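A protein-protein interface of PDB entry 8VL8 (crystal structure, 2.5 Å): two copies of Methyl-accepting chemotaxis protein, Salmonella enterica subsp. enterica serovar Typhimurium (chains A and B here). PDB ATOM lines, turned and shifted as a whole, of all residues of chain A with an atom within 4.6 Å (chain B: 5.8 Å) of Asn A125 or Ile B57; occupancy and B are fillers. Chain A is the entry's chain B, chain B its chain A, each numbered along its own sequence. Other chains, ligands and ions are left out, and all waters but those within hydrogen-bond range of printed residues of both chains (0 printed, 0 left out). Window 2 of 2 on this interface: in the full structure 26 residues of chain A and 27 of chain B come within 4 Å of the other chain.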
ATOM      1  N   MET A  51       8.702  22.979   8.689  1.00  0.00           N
ATOM      2  CA  MET A  51       9.189  23.782   9.787  1.00  0.00           C
ATOM      3  C   MET A  51       8.352  25.010   9.947  1.00  0.00           C
ATOM      4  O   MET A  51       7.963  25.353  11.069  1.00  0.00           O
ATOM      5  CB  MET A  51      10.663  24.102   9.580  1.00  0.00           C
ATOM      6  CG  MET A  51      11.509  22.822   9.911  1.00  0.00           C
ATOM      7  SD  MET A  51      11.456  22.440  11.706  1.00  0.00           S
ATOM      8  CE  MET A  51      12.102  24.025  12.315  1.00  0.00           C
ATOM      9  N   LYS A 123       9.601  13.543  11.029  1.00  0.00           N
ATOM     10  CA  LYS A 123      10.936  13.225  11.531  1.00  0.00           C
ATOM     11  C   LYS A 123      11.986  14.163  10.951  1.00  0.00           C
ATOM     12  O   LYS A 123      12.897  13.757  10.232  1.00  0.00           O
ATOM     13  CB  LYS A 123      11.287  11.773  11.231  1.00  0.00           C
ATOM     14  CG  LYS A 123      10.788  10.825  12.275  1.00  0.00           C
ATOM     15  CD  LYS A 123      10.894   9.395  11.779  1.00  0.00           C
ATOM     16  CE  LYS A 123      10.353   8.382  12.779  1.00  0.00           C
ATOM     17  NZ  LYS A 123      10.324   7.027  12.153  1.00  0.00           N
ATOM     18  N   ILE A 124      11.920  15.416  11.395  1.00  0.00           N
ATOM     19  CA  ILE A 124      12.651  16.473  10.687  1.00  0.00           C
ATOM     20  C   ILE A 124      14.158  16.371  10.897  1.00  0.00           C
ATOM     21  O   ILE A 124      14.929  16.685   9.977  1.00  0.00           O
ATOM     22  CB  ILE A 124      12.118  17.862  11.097  1.00  0.00           C
ATOM     23  CG1 ILE A 124      12.863  18.998  10.373  1.00  0.00           C
ATOM     24  CG2 ILE A 124      12.256  18.131  12.618  1.00  0.00           C
ATOM     25  CD1 ILE A 124      12.276  19.327   9.020  1.00  0.00           C
ATOM     26  N   ASN A 125      14.608  15.933  12.085  1.00  0.00           N
ATOM     27  CA  ASN A 125      16.049  15.865  12.351  1.00  0.00           C
ATOM     28  C   ASN A 125      16.686  14.716  11.585  1.00  0.00           C
ATOM     29  O   ASN A 125      17.754  14.881  10.955  1.00  0.00           O
ATOM     30  CB  ASN A 125      16.302  15.736  13.858  1.00  0.00           C
ATOM     31  CG  ASN A 125      15.965  17.028  14.625  1.00  0.00           C
ATOM     32  OD1 ASN A 125      16.805  17.925  14.785  1.00  0.00           O
ATOM     33  ND2 ASN A 125      14.697  17.159  15.011  1.00  0.00           N
ATOM     34  N   GLU A 126      16.033  13.547  11.616  1.00  0.00           N
ATOM     35  CA  GLU A 126      16.455  12.414  10.788  1.00  0.00           C
ATOM     36  C   GLU A 126      16.405  12.758   9.288  1.00  0.00           C
ATOM     37  O   GLU A 126      17.212  12.253   8.490  1.00  0.00           O
ATOM     38  CB  GLU A 126      15.546  11.214  11.049  1.00  0.00           C
ATOM     39  CG  GLU A 126      15.575  10.548  12.437  1.00  0.00           C
ATOM     40  CD  GLU A 126      14.934   9.168  12.344  1.00  0.00           C
ATOM     41  OE1 GLU A 126      15.342   8.368  11.449  1.00  0.00           O
ATOM     42  OE2 GLU A 126      13.996   8.901  13.121  1.00  0.00           O
ATOM     43  N   PHE A 127      15.405  13.546   8.884  1.00  0.00           N
ATOM     44  CA  PHE A 127      15.367  14.120   7.534  1.00  0.00           C
ATOM     45  C   PHE A 127      16.613  14.961   7.291  1.00  0.00           C
ATOM     46  O   PHE A 127      17.388  14.714   6.355  1.00  0.00           O
ATOM     47  CB  PHE A 127      14.097  14.995   7.370  1.00  0.00           C
ATOM     48  CG  PHE A 127      13.909  15.585   5.984  1.00  0.00           C
ATOM     49  CD1 PHE A 127      13.209  14.888   5.017  1.00  0.00           C
ATOM     50  CD2 PHE A 127      14.402  16.834   5.674  1.00  0.00           C
ATOM     51  CE1 PHE A 127      13.021  15.406   3.762  1.00  0.00           C
ATOM     52  CE2 PHE A 127      14.233  17.368   4.417  1.00  0.00           C
ATOM     53  CZ  PHE A 127      13.548  16.635   3.441  1.00  0.00           C
ATOM     54  N   PHE A 128      16.821  15.981   8.134  1.00  0.00           N
ATOM     55  CA  PHE A 128      17.889  16.929   7.818  1.00  0.00           C
ATOM     56  C   PHE A 128      19.267  16.302   7.935  1.00  0.00           C
ATOM     57  O   PHE A 128      20.188  16.688   7.189  1.00  0.00           O
ATOM     58  CB  PHE A 128      17.795  18.144   8.708  1.00  0.00           C
ATOM     59  CG  PHE A 128      18.738  19.209   8.352  1.00  0.00           C
ATOM     60  CD1 PHE A 128      18.399  20.158   7.379  1.00  0.00           C
ATOM     61  CD2 PHE A 128      20.006  19.248   8.917  1.00  0.00           C
ATOM     62  CE1 PHE A 128      19.297  21.169   7.022  1.00  0.00           C
ATOM     63  CE2 PHE A 128      20.891  20.275   8.603  1.00  0.00           C
ATOM     64  CZ  PHE A 128      20.553  21.224   7.632  1.00  0.00           C
ATOM     65  N   ASP A 129      19.407  15.299   8.812  1.00  0.00           N
ATOM     66  CA  ASP A 129      20.703  14.677   9.098  1.00  0.00           C
ATOM     67  C   ASP A 129      21.123  13.661   8.048  1.00  0.00           C
ATOM     68  O   ASP A 129      22.329  13.469   7.824  1.00  0.00           O
ATOM     69  CB  ASP A 129      20.664  13.955  10.449  1.00  0.00           C
ATOM     70  CG  ASP A 129      20.619  14.912  11.634  1.00  0.00           C
ATOM     71  OD1 ASP A 129      20.689  16.137  11.421  1.00  0.00           O
ATOM     72  OD2 ASP A 129      20.482  14.430  12.770  1.00  0.00           O
ATOM     73  N   ARG B  49      17.969  24.489   7.953  1.00  0.00           N
ATOM     74  CA  ARG B  49      18.834  24.748   9.100  1.00  0.00           C
ATOM     75  C   ARG B  49      18.540  26.089   9.715  1.00  0.00           C
ATOM     76  O   ARG B  49      18.481  26.207  10.950  1.00  0.00           O
ATOM     77  CB  ARG B  49      20.304  24.678   8.703  1.00  0.00           C
ATOM     78  CG  ARG B  49      21.286  24.821   9.908  1.00  0.00           C
ATOM     79  CD  ARG B  49      21.058  23.750  11.028  1.00  0.00           C
ATOM     80  NE  ARG B  49      21.590  24.223  12.317  1.00  0.00           N
ATOM     81  CZ  ARG B  49      22.743  23.840  12.869  1.00  0.00           C
ATOM     82  NH1 ARG B  49      23.477  22.863  12.355  1.00  0.00           N
ATOM     83  NH2 ARG B  49      23.180  24.469  13.950  1.00  0.00           N
ATOM     84  N   MET B  52      15.420  25.625  11.762  1.00  0.00           N
ATOM     85  CA  MET B  52      15.760  24.880  12.968  1.00  0.00           C
ATOM     86  C   MET B  52      16.468  25.752  13.984  1.00  0.00           C
ATOM     87  O   MET B  52      16.160  25.719  15.173  1.00  0.00           O
ATOM     88  CB  MET B  52      16.667  23.762  12.575  1.00  0.00           C
ATOM     89  CG  MET B  52      15.906  22.690  11.953  1.00  0.00           C
ATOM     90  SD  MET B  52      17.231  21.891  11.156  1.00  0.00           S
ATOM     91  CE  MET B  52      16.753  20.235  11.492  1.00  0.00           C
ATOM     92  N   ASP B  53      17.448  26.515  13.540  1.00  0.00           N
ATOM     93  CA  ASP B  53      18.163  27.336  14.494  1.00  0.00           C
ATOM     94  C   ASP B  53      17.196  28.257  15.241  1.00  0.00           C
ATOM     95  O   ASP B  53      17.333  28.457  16.452  1.00  0.00           O
ATOM     96  CB  ASP B  53      19.244  28.120  13.756  1.00  0.00           C
ATOM     97  CG  ASP B  53      20.457  27.281  13.414  1.00  0.00           C
ATOM     98  OD1 ASP B  53      20.558  26.075  13.772  1.00  0.00           O
ATOM     99  OD2 ASP B  53      21.327  27.866  12.739  1.00  0.00           O
ATOM    100  N   GLN B  54      16.200  28.815  14.540  1.00  0.00           N
ATOM    101  CA  GLN B  54      15.165  29.599  15.210  1.00  0.00           C
ATOM    102  C   GLN B  54      14.447  28.797  16.288  1.00  0.00           C
ATOM    103  O   GLN B  54      14.021  29.366  17.302  1.00  0.00           O
ATOM    104  CB  GLN B  54      14.116  30.115  14.226  1.00  0.00           C
ATOM    105  CG  GLN B  54      14.667  30.579  12.923  1.00  0.00           C
ATOM    106  CD  GLN B  54      15.841  31.515  13.123  1.00  0.00           C
ATOM    107  OE1 GLN B  54      17.005  31.171  12.806  1.00  0.00           O
ATOM    108  NE2 GLN B  54      15.561  32.698  13.644  1.00  0.00           N
ATOM    109  N   SER B  55      14.256  27.501  16.084  1.00  0.00           N
ATOM    110  CA  SER B  55      13.605  26.686  17.099  1.00  0.00           C
ATOM    111  C   SER B  55      14.617  25.945  17.957  1.00  0.00           C
ATOM    112  O   SER B  55      14.245  25.026  18.685  1.00  0.00           O
ATOM    113  CB  SER B  55      12.631  25.699  16.454  1.00  0.00           C
ATOM    114  OG  SER B  55      13.157  25.189  15.241  1.00  0.00           O
ATOM    115  N   ASN B  56      15.888  26.323  17.858  1.00  0.00           N
ATOM    116  CA  ASN B  56      16.988  25.721  18.595  1.00  0.00           C
ATOM    117  C   ASN B  56      16.936  24.205  18.561  1.00  0.00           C
ATOM    118  O   ASN B  56      17.046  23.528  19.581  1.00  0.00           O
ATOM    119  CB  ASN B  56      17.014  26.246  20.029  1.00  0.00           C
ATOM    120  CG  ASN B  56      17.313  27.716  20.081  1.00  0.00           C
ATOM    121  OD1 ASN B  56      18.453  28.125  19.854  1.00  0.00           O
ATOM    122  ND2 ASN B  56      16.296  28.530  20.445  1.00  0.00           N
ATOM    123  N   ILE B  57      16.787  23.664  17.357  1.00  0.00           N
ATOM    124  CA  ILE B  57      16.867  22.222  17.184  1.00  0.00           C
ATOM    125  C   ILE B  57      17.865  21.945  16.080  1.00  0.00           C
ATOM    126  O   ILE B  57      17.899  20.856  15.511  1.00  0.00           O
ATOM    127  CB  ILE B  57      15.487  21.624  16.909  1.00  0.00           C
ATOM    128  CG1 ILE B  57      15.017  21.863  15.482  1.00  0.00           C
ATOM    129  CG2 ILE B  57      14.495  22.250  17.874  1.00  0.00           C
ATOM    130  CD1 ILE B  57      13.534  21.438  15.319  1.00  0.00           C
ATOM    131  N   GLY B  58      18.753  22.914  15.873  1.00  0.00           N
ATOM    132  CA  GLY B  58      19.748  22.797  14.833  1.00  0.00           C
ATOM    133  C   GLY B  58      20.636  21.579  14.993  1.00  0.00           C
ATOM    134  O   GLY B  58      20.880  21.088  16.087  1.00  0.00           O
ATOM    135  N   SER B  59      21.135  21.098  13.865  1.00  0.00           N
ATOM    136  CA  SER B  59      21.937  19.886  13.798  1.00  0.00           C
ATOM    137  C   SER B  59      22.492  19.779  12.383  1.00  0.00           C
ATOM    138  O   SER B  59      22.005  20.431  11.449  1.00  0.00           O
ATOM    139  CB  SER B  59      21.132  18.618  14.179  1.00  0.00           C
ATOM    140  OG  SER B  59      19.936  18.393  13.411  1.00  0.00           O
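Among the printed residues, pairs that only touch across the chains: Phe A128 with Ser B59 (3.1 Å), Met A51 with Ser B55 (3.3 Å), Phe A128 with Arg B49 (3.6 Å), Phe A128 with Met B52 (3.6 Å) and Met A51 with Met B52 (3.7 Å).
Of the 8 printed residues of chain A, 4 touch a printed residue of chain B. Printed residues of chain A that touch a printed residue of chain B: Met A51, Asn A125, Phe A128 and Asp A129. Hydrophobic or aromatic side chains of chain A within 4 Å of the printed part of chain B: Met A51 and Phe A128. Of the 9 printed residues of chain B, 5 touch a printed residue of chain A. Hydrophobic or aromatic side chains of chain B within 4 Å of the printed part of chain A: Met B52. Among the printed residues, no Asp or Glu carboxylate lies within 4 Å of a Lys or Arg side-chain nitrogen of the other chain.
The guanidinium group (NH1) of Arg B49 is in hydrogen-bond range of the backbone carbonyl oxygen (O) of Ser B59 (3.0 Å). OG of Ser B55 lies within hydrogen-bond range of O of Met B52 (3.1 Å). NE of Arg B49 is in salt-bridge range of OD1 of Asp B53 (2.6 Å). O of Met B52 is in hydrogen-bond range of N of Ile B57 (3.1 Å).
No position is printed for both chains. Of the 8 pairs that touch across the chains among the printed residues, none has its exchanged pair printed and touching as well.
Of the printed residues of chain B, Asn A125 touches Ile B57 (3.2 Å) and Ser B59 (3.5 Å). Ile B57 touches just one residue of chain A: Asn A125. Printed residues of chain A within 4 Å of Ser B55: Met A51. Printed residues of chain B within 4 Å of Asp A129: Ser B59 (3.1 Å). Glu A126 touches none of the printed residues of chain B. Gly B58 touches none of the printed residues of chain A. The nearest residue of chain B that does not touch Asn A125 is Met B52 (4.02 Å).
The side-chain hydroxyl (OG) of Ser B59 sits at hydrogen-bond distance from the side-chain carboxylate (OD1) of Asp A129 (3.1 Å). OD1 of Asn A125 lies close to O of Ile B57. The side-chain hydroxyl (OG) of Ser B59 lies within hydrogen-bond range of the side-chain amide oxygen (OD1) of Asn A125, 3.5 Å away.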
